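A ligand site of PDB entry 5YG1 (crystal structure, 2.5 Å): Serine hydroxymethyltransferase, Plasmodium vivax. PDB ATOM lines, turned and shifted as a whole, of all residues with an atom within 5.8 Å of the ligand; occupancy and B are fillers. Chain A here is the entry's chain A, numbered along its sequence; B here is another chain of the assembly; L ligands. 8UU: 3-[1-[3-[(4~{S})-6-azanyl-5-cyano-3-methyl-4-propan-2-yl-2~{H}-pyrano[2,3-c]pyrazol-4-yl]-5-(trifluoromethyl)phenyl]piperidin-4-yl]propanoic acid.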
ATOM      1  N   HIS A 123     -13.008  22.040 -31.194  1.00  0.00           N
ATOM      2  CA  HIS A 123     -13.261  21.331 -29.946  1.00  0.00           C
ATOM      3  C   HIS A 123     -13.785  22.319 -28.897  1.00  0.00           C
ATOM      4  O   HIS A 123     -13.431  23.515 -28.913  1.00  0.00           O
ATOM      5  CB  HIS A 123     -11.961  20.706 -29.460  1.00  0.00           C
ATOM      6  CG  HIS A 123     -12.143  19.568 -28.527  1.00  0.00           C
ATOM      7  ND1 HIS A 123     -12.344  19.749 -27.179  1.00  0.00           N
ATOM      8  CD2 HIS A 123     -12.146  18.230 -28.731  1.00  0.00           C
ATOM      9  CE1 HIS A 123     -12.463  18.567 -26.580  1.00  0.00           C
ATOM     10  NE2 HIS A 123     -12.367  17.634 -27.508  1.00  0.00           N
ATOM     11  N   LEU A 124     -14.651  21.822 -28.010  1.00  0.00           N
ATOM     12  CA  LEU A 124     -15.241  22.633 -26.933  1.00  0.00           C
ATOM     13  C   LEU A 124     -14.159  23.262 -26.060  1.00  0.00           C
ATOM     14  O   LEU A 124     -14.170  24.470 -25.837  1.00  0.00           O
ATOM     15  CB  LEU A 124     -16.176  21.785 -26.077  1.00  0.00           C
ATOM     16  CG  LEU A 124     -16.847  22.507 -24.895  1.00  0.00           C
ATOM     17  CD1 LEU A 124     -18.310  22.836 -25.179  1.00  0.00           C
ATOM     18  CD2 LEU A 124     -16.731  21.663 -23.636  1.00  0.00           C
ATOM     19  N   CYS A 125     -13.250  22.408 -25.564  1.00  0.00           N
ATOM     20  CA  CYS A 125     -12.007  22.799 -24.843  1.00  0.00           C
ATOM     21  C   CYS A 125     -11.104  23.856 -25.504  1.00  0.00           C
ATOM     22  O   CYS A 125     -10.290  24.477 -24.810  1.00  0.00           O
ATOM     23  CB  CYS A 125     -11.161  21.564 -24.489  1.00  0.00           C
ATOM     24  SG  CYS A 125     -11.991  20.301 -23.477  1.00  0.00           S
ATOM     25  N   SER A 126     -11.200  24.047 -26.819  1.00  0.00           N
ATOM     26  CA  SER A 126     -10.447  25.094 -27.517  1.00  0.00           C
ATOM     27  C   SER A 126     -11.282  26.323 -27.867  1.00  0.00           C
ATOM     28  O   SER A 126     -10.757  27.289 -28.445  1.00  0.00           O
ATOM     29  CB  SER A 126      -9.839  24.524 -28.789  1.00  0.00           C
ATOM     30  OG  SER A 126      -9.012  23.401 -28.515  1.00  0.00           O
ATOM     31  N   GLY A 127     -12.573  26.304 -27.515  1.00  0.00           N
ATOM     32  CA  GLY A 127     -13.460  27.444 -27.743  1.00  0.00           C
ATOM     33  C   GLY A 127     -14.645  27.179 -28.658  1.00  0.00           C
ATOM     34  O   GLY A 127     -15.446  28.061 -28.881  1.00  0.00           O
ATOM     35  N   GLY A 128     -14.787  25.966 -29.187  1.00  0.00           N
ATOM     36  CA  GLY A 128     -15.953  25.624 -29.983  1.00  0.00           C
ATOM     37  C   GLY A 128     -17.215  25.438 -29.157  1.00  0.00           C
ATOM     38  O   GLY A 128     -17.164  25.255 -27.936  1.00  0.00           O
ATOM     39  N   HIS A 129     -18.368  25.521 -29.844  1.00  0.00           N
ATOM     40  CA  HIS A 129     -19.653  25.234 -29.228  1.00  0.00           C
ATOM     41  C   HIS A 129     -19.995  23.765 -29.235  1.00  0.00           C
ATOM     42  O   HIS A 129     -19.445  22.981 -30.002  1.00  0.00           O
ATOM     43  CB  HIS A 129     -20.763  26.016 -29.916  1.00  0.00           C
ATOM     44  CG  HIS A 129     -21.977  26.198 -29.044  1.00  0.00           C
ATOM     45  ND1 HIS A 129     -23.190  25.605 -29.332  1.00  0.00           N
ATOM     46  CD2 HIS A 129     -22.144  26.847 -27.871  1.00  0.00           C
ATOM     47  CE1 HIS A 129     -24.060  25.903 -28.387  1.00  0.00           C
ATOM     48  NE2 HIS A 129     -23.453  26.667 -27.489  1.00  0.00           N
ATOM     49  N   LEU A 130     -20.935  23.401 -28.368  1.00  0.00           N
ATOM     50  CA  LEU A 130     -21.505  22.055 -28.320  1.00  0.00           C
ATOM     51  C   LEU A 130     -22.096  21.612 -29.652  1.00  0.00           C
ATOM     52  O   LEU A 130     -21.983  20.441 -30.036  1.00  0.00           O
ATOM     53  CB  LEU A 130     -22.625  22.008 -27.286  1.00  0.00           C
ATOM     54  CG  LEU A 130     -22.157  22.272 -25.868  1.00  0.00           C
ATOM     55  CD1 LEU A 130     -23.330  22.747 -25.042  1.00  0.00           C
ATOM     56  CD2 LEU A 130     -21.511  21.025 -25.296  1.00  0.00           C
ATOM     57  N   PHE A 134     -19.440  18.477 -30.839  1.00  0.00           N
ATOM     58  CA  PHE A 134     -18.718  18.062 -29.645  1.00  0.00           C
ATOM     59  C   PHE A 134     -19.096  16.684 -29.137  1.00  0.00           C
ATOM     60  O   PHE A 134     -20.276  16.425 -28.907  1.00  0.00           O
ATOM     61  CB  PHE A 134     -18.893  19.024 -28.479  1.00  0.00           C
ATOM     62  CG  PHE A 134     -18.153  18.575 -27.269  1.00  0.00           C
ATOM     63  CD1 PHE A 134     -16.753  18.470 -27.304  1.00  0.00           C
ATOM     64  CD2 PHE A 134     -18.837  18.139 -26.143  1.00  0.00           C
ATOM     65  CE1 PHE A 134     -16.062  17.984 -26.199  1.00  0.00           C
ATOM     66  CE2 PHE A 134     -18.146  17.653 -25.037  1.00  0.00           C
ATOM     67  CZ  PHE A 134     -16.761  17.576 -25.055  1.00  0.00           C
ATOM     68  N   VAL A 141     -21.805  13.711 -26.847  1.00  0.00           N
ATOM     69  CA  VAL A 141     -22.440  14.700 -25.969  1.00  0.00           C
ATOM     70  C   VAL A 141     -23.485  15.541 -26.694  1.00  0.00           C
ATOM     71  O   VAL A 141     -24.555  15.789 -26.159  1.00  0.00           O
ATOM     72  CB  VAL A 141     -21.361  15.613 -25.308  1.00  0.00           C
ATOM     73  CG1 VAL A 141     -21.984  16.746 -24.503  1.00  0.00           C
ATOM     74  CG2 VAL A 141     -20.446  14.778 -24.409  1.00  0.00           C
ATOM     75  N   THR A 183     -17.351  29.913 -29.403  1.00  0.00           N
ATOM     76  CA  THR A 183     -18.030  30.341 -28.176  1.00  0.00           C
ATOM     77  C   THR A 183     -17.101  31.136 -27.262  1.00  0.00           C
ATOM     78  O   THR A 183     -17.532  32.187 -26.737  1.00  0.00           O
ATOM     79  CB  THR A 183     -18.869  29.238 -27.447  1.00  0.00           C
ATOM     80  OG1 THR A 183     -18.439  29.052 -26.081  1.00  0.00           O
ATOM     81  CG2 THR A 183     -18.789  27.977 -28.106  1.00  0.00           C
ATOM     82  N   SER A 184     -15.853  30.714 -27.122  1.00  0.00           N
ATOM     83  CA  SER A 184     -14.898  31.475 -26.314  1.00  0.00           C
ATOM     84  C   SER A 184     -13.511  31.625 -26.933  1.00  0.00           C
ATOM     85  O   SER A 184     -12.515  31.215 -26.392  1.00  0.00           O
ATOM     86  CB  SER A 184     -14.821  30.887 -24.894  1.00  0.00           C
ATOM     87  OG  SER A 184     -14.681  29.485 -24.928  1.00  0.00           O
ATOM     88  N   ASN A 354     -17.848  33.080 -16.036  1.00  0.00           N
ATOM     89  CA  ASN A 354     -17.931  31.630 -16.155  1.00  0.00           C
ATOM     90  C   ASN A 354     -16.566  31.024 -16.241  1.00  0.00           C
ATOM     91  O   ASN A 354     -15.660  31.605 -16.822  1.00  0.00           O
ATOM     92  CB  ASN A 354     -18.822  31.183 -17.314  1.00  0.00           C
ATOM     93  CG  ASN A 354     -18.283  31.572 -18.671  1.00  0.00           C
ATOM     94  OD1 ASN A 354     -18.646  32.628 -19.201  1.00  0.00           O
ATOM     95  ND2 ASN A 354     -17.418  30.730 -19.227  1.00  0.00           N
ATOM     96  N   LYS A 355     -16.440  29.847 -15.633  1.00  0.00           N
ATOM     97  CA  LYS A 355     -15.265  29.035 -15.804  1.00  0.00           C
ATOM     98  C   LYS A 355     -15.092  28.644 -17.279  1.00  0.00           C
ATOM     99  O   LYS A 355     -16.043  28.510 -18.046  1.00  0.00           O
ATOM    100  CB  LYS A 355     -15.288  27.775 -14.912  1.00  0.00           C
ATOM    101  CG  LYS A 355     -16.629  27.050 -14.838  1.00  0.00           C
ATOM    102  CD  LYS A 355     -16.504  25.614 -14.401  1.00  0.00           C
ATOM    103  CE  LYS A 355     -17.882  24.974 -14.296  1.00  0.00           C
ATOM    104  NZ  LYS A 355     -17.812  23.624 -13.658  1.00  0.00           N
ATOM    105  N   ASN A 356     -13.838  28.457 -17.678  1.00  0.00           N
ATOM    106  CA  ASN A 356     -13.512  28.218 -19.056  1.00  0.00           C
ATOM    107  C   ASN A 356     -12.218  27.441 -19.146  1.00  0.00           C
ATOM    108  O   ASN A 356     -11.294  27.601 -18.345  1.00  0.00           O
ATOM    109  CB  ASN A 356     -13.411  29.559 -19.806  1.00  0.00           C
ATOM    110  CG  ASN A 356     -13.848  29.449 -21.261  1.00  0.00           C
ATOM    111  OD1 ASN A 356     -14.997  29.746 -21.590  1.00  0.00           O
ATOM    112  ND2 ASN A 356     -12.963  28.984 -22.117  1.00  0.00           N
ATOM    113  N   THR A 357     -12.153  26.596 -20.156  1.00  0.00           N
ATOM    114  CA  THR A 357     -10.971  25.816 -20.449  1.00  0.00           C
ATOM    115  C   THR A 357      -9.862  26.667 -21.087  1.00  0.00           C
ATOM    116  O   THR A 357     -10.123  27.753 -21.634  1.00  0.00           O
ATOM    117  CB  THR A 357     -11.350  24.667 -21.387  1.00  0.00           C
ATOM    118  OG1 THR A 357     -12.102  25.197 -22.488  1.00  0.00           O
ATOM    119  CG2 THR A 357     -12.229  23.669 -20.638  1.00  0.00           C
ATOM    120  N   ASP A 363      -8.920  18.002 -19.725  1.00  0.00           N
ATOM    121  CA  ASP A 363     -10.294  17.638 -19.398  1.00  0.00           C
ATOM    122  C   ASP A 363     -11.098  18.862 -18.916  1.00  0.00           C
ATOM    123  O   ASP A 363     -10.575  19.746 -18.247  1.00  0.00           O
ATOM    124  CB  ASP A 363     -10.281  16.510 -18.345  1.00  0.00           C
ATOM    125  CG  ASP A 363     -11.670  15.928 -18.048  1.00  0.00           C
ATOM    126  OD1 ASP A 363     -12.561  15.950 -18.927  1.00  0.00           O
ATOM    127  OD2 ASP A 363     -11.859  15.429 -16.911  1.00  0.00           O
ATOM    128  N   CYS A 364     -12.385  18.881 -19.274  1.00  0.00           N
ATOM    129  CA  CYS A 364     -13.329  19.946 -18.887  1.00  0.00           C
ATOM    130  C   CYS A 364     -13.702  20.022 -17.394  1.00  0.00           C
ATOM    131  O   CYS A 364     -14.319  20.994 -16.975  1.00  0.00           O
ATOM    132  CB  CYS A 364     -14.621  19.825 -19.697  1.00  0.00           C
ATOM    133  SG  CYS A 364     -14.366  20.204 -21.433  1.00  0.00           S
ATOM    134  N   VAL A 365     -13.380  18.977 -16.616  1.00  0.00           N
ATOM    135  CA  VAL A 365     -13.460  19.039 -15.154  1.00  0.00           C
ATOM    136  C   VAL A 365     -12.160  19.698 -14.691  1.00  0.00           C
ATOM    137  O   VAL A 365     -11.072  19.324 -15.169  1.00  0.00           O
ATOM    138  CB  VAL A 365     -13.605  17.647 -14.465  1.00  0.00           C
ATOM    139  CG1 VAL A 365     -14.155  17.818 -13.048  1.00  0.00           C
ATOM    140  CG2 VAL A 365     -14.526  16.700 -15.241  1.00  0.00           C
ATOM    141  N   SER A 366     -12.273  20.665 -13.789  1.00  0.00           N
ATOM    142  CA  SER A 366     -11.134  21.501 -13.358  1.00  0.00           C
ATOM    143  C   SER A 366     -10.485  22.314 -14.510  1.00  0.00           C
ATOM    144  O   SER A 366      -9.290  22.152 -14.790  1.00  0.00           O
ATOM    145  CB  SER A 366     -10.091  20.619 -12.612  1.00  0.00           C
ATOM    146  OG  SER A 366      -8.919  21.353 -12.265  1.00  0.00           O
ATOM    147  N   PRO A 367     -11.268  23.189 -15.202  1.00  0.00           N
ATOM    148  CA  PRO A 367     -10.690  24.078 -16.209  1.00  0.00           C
ATOM    149  C   PRO A 367      -9.832  25.172 -15.564  1.00  0.00           C
ATOM    150  O   PRO A 367     -10.143  25.612 -14.443  1.00  0.00           O
ATOM    151  CB  PRO A 367     -11.907  24.703 -16.859  1.00  0.00           C
ATOM    152  CG  PRO A 367     -12.893  24.757 -15.764  1.00  0.00           C
ATOM    153  CD  PRO A 367     -12.716  23.423 -15.099  1.00  0.00           C
ATOM    154  N   ARG A 371     -13.709  33.167 -18.326  1.00  0.00           N
ATOM    155  CA  ARG A 371     -13.941  33.985 -19.469  1.00  0.00           C
ATOM    156  C   ARG A 371     -14.790  35.176 -19.070  1.00  0.00           C
ATOM    157  O   ARG A 371     -15.798  35.015 -18.388  1.00  0.00           O
ATOM    158  CB  ARG A 371     -14.667  33.159 -20.508  1.00  0.00           C
ATOM    159  CG  ARG A 371     -15.059  33.903 -21.782  1.00  0.00           C
ATOM    160  CD  ARG A 371     -16.051  33.060 -22.546  1.00  0.00           C
ATOM    161  NE  ARG A 371     -17.389  33.130 -21.991  1.00  0.00           N
ATOM    162  CZ  ARG A 371     -18.494  32.649 -22.574  1.00  0.00           C
ATOM    163  NH1 ARG A 371     -18.445  32.066 -23.756  1.00  0.00           N
ATOM    164  NH2 ARG A 371     -19.667  32.757 -21.947  1.00  0.00           N
ATOM    165  N   GLU B  56     -27.376  27.456 -18.539  1.00  0.00           N
ATOM    166  CA  GLU B  56     -27.161  26.106 -19.050  1.00  0.00           C
ATOM    167  C   GLU B  56     -27.059  25.063 -17.946  1.00  0.00           C
ATOM    168  O   GLU B  56     -26.424  25.288 -16.939  1.00  0.00           O
ATOM    169  CB  GLU B  56     -25.926  26.066 -19.940  1.00  0.00           C
ATOM    170  CG  GLU B  56     -26.258  26.379 -21.397  1.00  0.00           C
ATOM    171  CD  GLU B  56     -25.062  26.796 -22.233  1.00  0.00           C
ATOM    172  OE1 GLU B  56     -24.673  27.966 -22.086  1.00  0.00           O
ATOM    173  OE2 GLU B  56     -24.539  25.989 -23.038  1.00  0.00           O
ATOM    174  N   TYR B  63     -23.929  25.711 -14.890  1.00  0.00           N
ATOM    175  CA  TYR B  63     -22.550  25.935 -15.265  1.00  0.00           C
ATOM    176  C   TYR B  63     -22.109  27.192 -14.602  1.00  0.00           C
ATOM    177  O   TYR B  63     -21.071  27.207 -13.935  1.00  0.00           O
ATOM    178  CB  TYR B  63     -22.348  25.883 -16.801  1.00  0.00           C
ATOM    179  CG  TYR B  63     -22.241  24.428 -17.161  1.00  0.00           C
ATOM    180  CD1 TYR B  63     -23.389  23.642 -17.265  1.00  0.00           C
ATOM    181  CD2 TYR B  63     -21.006  23.795 -17.207  1.00  0.00           C
ATOM    182  CE1 TYR B  63     -23.306  22.278 -17.478  1.00  0.00           C
ATOM    183  CE2 TYR B  63     -20.920  22.422 -17.419  1.00  0.00           C
ATOM    184  CZ  TYR B  63     -22.066  21.685 -17.554  1.00  0.00           C
ATOM    185  OH  TYR B  63     -22.007  20.325 -17.763  1.00  0.00           O
ATOM    186  N   TYR B  64     -22.928  28.239 -14.709  1.00  0.00           N
ATOM    187  CA  TYR B  64     -22.584  29.534 -14.101  1.00  0.00           C
ATOM    188  C   TYR B  64     -23.284  29.683 -12.752  1.00  0.00           C
ATOM    189  O   TYR B  64     -24.300  29.066 -12.517  1.00  0.00           O
ATOM    190  CB  TYR B  64     -22.989  30.711 -14.994  1.00  0.00           C
ATOM    191  CG  TYR B  64     -22.815  30.518 -16.482  1.00  0.00           C
ATOM    192  CD1 TYR B  64     -22.090  29.443 -17.026  1.00  0.00           C
ATOM    193  CD2 TYR B  64     -23.365  31.449 -17.365  1.00  0.00           C
ATOM    194  CE1 TYR B  64     -21.953  29.303 -18.391  1.00  0.00           C
ATOM    195  CE2 TYR B  64     -23.208  31.324 -18.746  1.00  0.00           C
ATOM    196  CZ  TYR B  64     -22.523  30.250 -19.259  1.00  0.00           C
ATOM    197  OH  TYR B  64     -22.387  30.119 -20.634  1.00  0.00           O
ATOM    198  N   SER B 263     -30.546  14.842 -20.210  1.00  0.00           N
ATOM    199  CA  SER B 263     -29.349  14.879 -21.050  1.00  0.00           C
ATOM    200  C   SER B 263     -29.706  15.182 -22.523  1.00  0.00           C
ATOM    201  O   SER B 263     -28.973  15.866 -23.209  1.00  0.00           O
ATOM    202  CB  SER B 263     -28.559  13.542 -20.904  1.00  0.00           C
ATOM    203  OG  SER B 263     -27.854  13.181 -22.063  1.00  0.00           O
ATOM    204  N   PHE B 266     -30.712  18.877 -22.639  1.00  0.00           N
ATOM    205  CA  PHE B 266     -29.384  19.484 -22.581  1.00  0.00           C
ATOM    206  C   PHE B 266     -28.358  18.514 -22.044  1.00  0.00           C
ATOM    207  O   PHE B 266     -28.636  17.876 -21.061  1.00  0.00           O
ATOM    208  CB  PHE B 266     -29.375  20.701 -21.683  1.00  0.00           C
ATOM    209  CG  PHE B 266     -28.003  21.313 -21.501  1.00  0.00           C
ATOM    210  CD1 PHE B 266     -27.524  22.219 -22.439  1.00  0.00           C
ATOM    211  CD2 PHE B 266     -27.194  20.969 -20.410  1.00  0.00           C
ATOM    212  CE1 PHE B 266     -26.281  22.797 -22.298  1.00  0.00           C
ATOM    213  CE2 PHE B 266     -25.941  21.573 -20.256  1.00  0.00           C
ATOM    214  CZ  PHE B 266     -25.481  22.482 -21.210  1.00  0.00           C
ATOM    215  N   PRO B 267     -27.173  18.435 -22.626  1.00  0.00           N
ATOM    216  CA  PRO B 267     -26.702  19.294 -23.689  1.00  0.00           C
ATOM    217  C   PRO B 267     -26.880  18.735 -25.083  1.00  0.00           C
ATOM    218  O   PRO B 267     -26.322  19.286 -26.026  1.00  0.00           O
ATOM    219  CB  PRO B 267     -25.222  19.383 -23.389  1.00  0.00           C
ATOM    220  CG  PRO B 267     -24.914  17.971 -22.979  1.00  0.00           C
ATOM    221  CD  PRO B 267     -26.140  17.448 -22.272  1.00  0.00           C
HETATM  222  F37 8UU L   1     -15.317  25.203 -18.129  1.00  0.00           F
HETATM  223  C21 8UU L   1     -16.044  24.078 -18.103  1.00  0.00           C
HETATM  224  F35 8UU L   1     -15.202  23.080 -18.115  1.00  0.00           F
HETATM  225  F36 8UU L   1     -16.756  23.862 -16.997  1.00  0.00           F
HETATM  226  C18 8UU L   1     -17.001  24.006 -19.295  1.00  0.00           C
HETATM  227  C17 8UU L   1     -17.251  25.101 -20.127  1.00  0.00           C
HETATM  228  C34 8UU L   1     -17.664  22.804 -19.519  1.00  0.00           C
HETATM  229  C19 8UU L   1     -18.561  22.672 -20.561  1.00  0.00           C
HETATM  230  N23 8UU L   1     -19.214  21.447 -20.835  1.00  0.00           N
HETATM  231  C28 8UU L   1     -18.401  20.209 -20.839  1.00  0.00           C
HETATM  232  C27 8UU L   1     -19.270  19.017 -20.486  1.00  0.00           C
HETATM  233  C26 8UU L   1     -20.580  19.084 -21.263  1.00  0.00           C
HETATM  234  C29 8UU L   1     -21.510  17.898 -20.987  1.00  0.00           C
HETATM  235  C30 8UU L   1     -20.925  16.545 -20.551  1.00  0.00           C
HETATM  236  C31 8UU L   1     -22.095  15.662 -20.154  1.00  0.00           C
HETATM  237  O33 8UU L   1     -22.609  14.861 -20.977  1.00  0.00           O
HETATM  238  O32 8UU L   1     -22.534  15.813 -18.988  1.00  0.00           O
HETATM  239  C25 8UU L   1     -21.357  20.281 -20.816  1.00  0.00           C
HETATM  240  C24 8UU L   1     -20.622  21.552 -21.214  1.00  0.00           C
HETATM  241  C20 8UU L   1     -18.775  23.766 -21.406  1.00  0.00           C
HETATM  242  C16 8UU L   1     -18.150  25.006 -21.212  1.00  0.00           C
HETATM  243  C4  8UU L   1     -18.408  26.184 -22.130  1.00  0.00           C
HETATM  244  C14 8UU L   1     -18.445  27.578 -21.432  1.00  0.00           C
HETATM  245  C22 8UU L   1     -18.857  28.761 -22.348  1.00  0.00           C
HETATM  246  C15 8UU L   1     -19.294  27.673 -20.150  1.00  0.00           C
HETATM  247  C3  8UU L   1     -17.279  26.203 -23.161  1.00  0.00           C
HETATM  248  C8  8UU L   1     -16.123  26.259 -22.682  1.00  0.00           C
HETATM  249  N9  8UU L   1     -15.051  26.258 -22.181  1.00  0.00           N
HETATM  250  C2  8UU L   1     -17.480  26.274 -24.499  1.00  0.00           C
HETATM  251  N7  8UU L   1     -16.473  26.343 -25.365  1.00  0.00           N
HETATM  252  C5  8UU L   1     -19.712  26.018 -22.829  1.00  0.00           C
HETATM  253  C10 8UU L   1     -21.113  25.805 -22.377  1.00  0.00           C
HETATM  254  C13 8UU L   1     -21.661  25.638 -20.984  1.00  0.00           C
HETATM  255  N11 8UU L   1     -21.848  25.759 -23.494  1.00  0.00           N
HETATM  256  N12 8UU L   1     -21.128  25.894 -24.700  1.00  0.00           N
HETATM  257  C6  8UU L   1     -19.882  26.078 -24.283  1.00  0.00           C
HETATM  258  O1  8UU L   1     -18.805  26.271 -25.072  1.00  0.00           O
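The side-chain amide nitrogen of Asn 356 sits at hydrogen-bond distance from a nitrogen (N9) of the ligand, at 3.4 Å. OE2 of Glu 56 of chain B sits at hydrogen-bond distance from N11 of the ligand, at 2.7 Å. The side-chain hydroxyl (OG1) of Thr 183 sits at hydrogen-bond distance from an oxygen (O1) of the ligand, at 3.0 Å. The side-chain hydroxyl (OG1) of Thr 357 is in hydrogen-bond range of a nitrogen (N9) of the ligand (3.1 Å). The backbone carbonyl oxygen (O) of Gly 128 sits at hydrogen-bond distance from a nitrogen (N7) of the ligand (2.9 Å). O of Leu 124 is in hydrogen-bond range of N7 of the ligand (3.0 Å).
O of Lys 355 lies close to F37 of the ligand, 3.4 Å away. A fluorine (F35) of the ligand sits close to the backbone carbonyl oxygen of Cys 364, at 2.5 Å. Residues that only touch the ligand: Tyr 63 of chain B, Pro 367, His 129, Tyr 64 of chain B, Arg 371, Ser 184, Leu 130, Asn 354, Val 141, Gly 127 and Pro 267 of chain B. Hydrophobic or aromatic side chains that line the ligand: Leu 124, His 129, Leu 130, Val 141, Pro 367, Tyr 63 of chain B, Tyr 64 of chain B and Pro 267 of chain B. 19 residues have an atom within 4 Å of the ligand: Leu 124, Gly 127, Gly 128, His 129, Leu 130, Val 141, Thr 183, Ser 184, Asn 354, Lys 355, Asn 356, Thr 357, Cys 364, Pro 367, Arg 371, Glu 56 of chain B, Tyr 63 of chain B, Tyr 64 of chain B and Pro 267 of chain B. The nearest printed residue that does not touch the ligand is Phe 266 of chain B (4.7 Å).
The backbone NH of Arg 371 sits at hydrogen-bond distance from the backbone carbonyl oxygen of Asn 354. The backbone carbonyl oxygen of Gly 127 lies within hydrogen-bond range of the backbone NH of Ser 184, at 3.2 Å. OG of Ser 184 sits at hydrogen-bond distance from ND2 of Asn 356. O of Thr 183 is in hydrogen-bond range of NH1 of Arg 371. OH of Tyr 64 of chain B sits at hydrogen-bond distance from OE1 of Glu 56 of chain B, at 3.5 Å. O of Cys 125 is in hydrogen-bond range of OG1 of Thr 357, 3.0 Å away. The backbone NH (N) of Gly 128 is in hydrogen-bond range of the backbone carbonyl oxygen (O) of His 123 (2.8 Å). O of Glu 56 of chain B sits at hydrogen-bond distance from N of Tyr 63 of chain B (3.3 Å).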
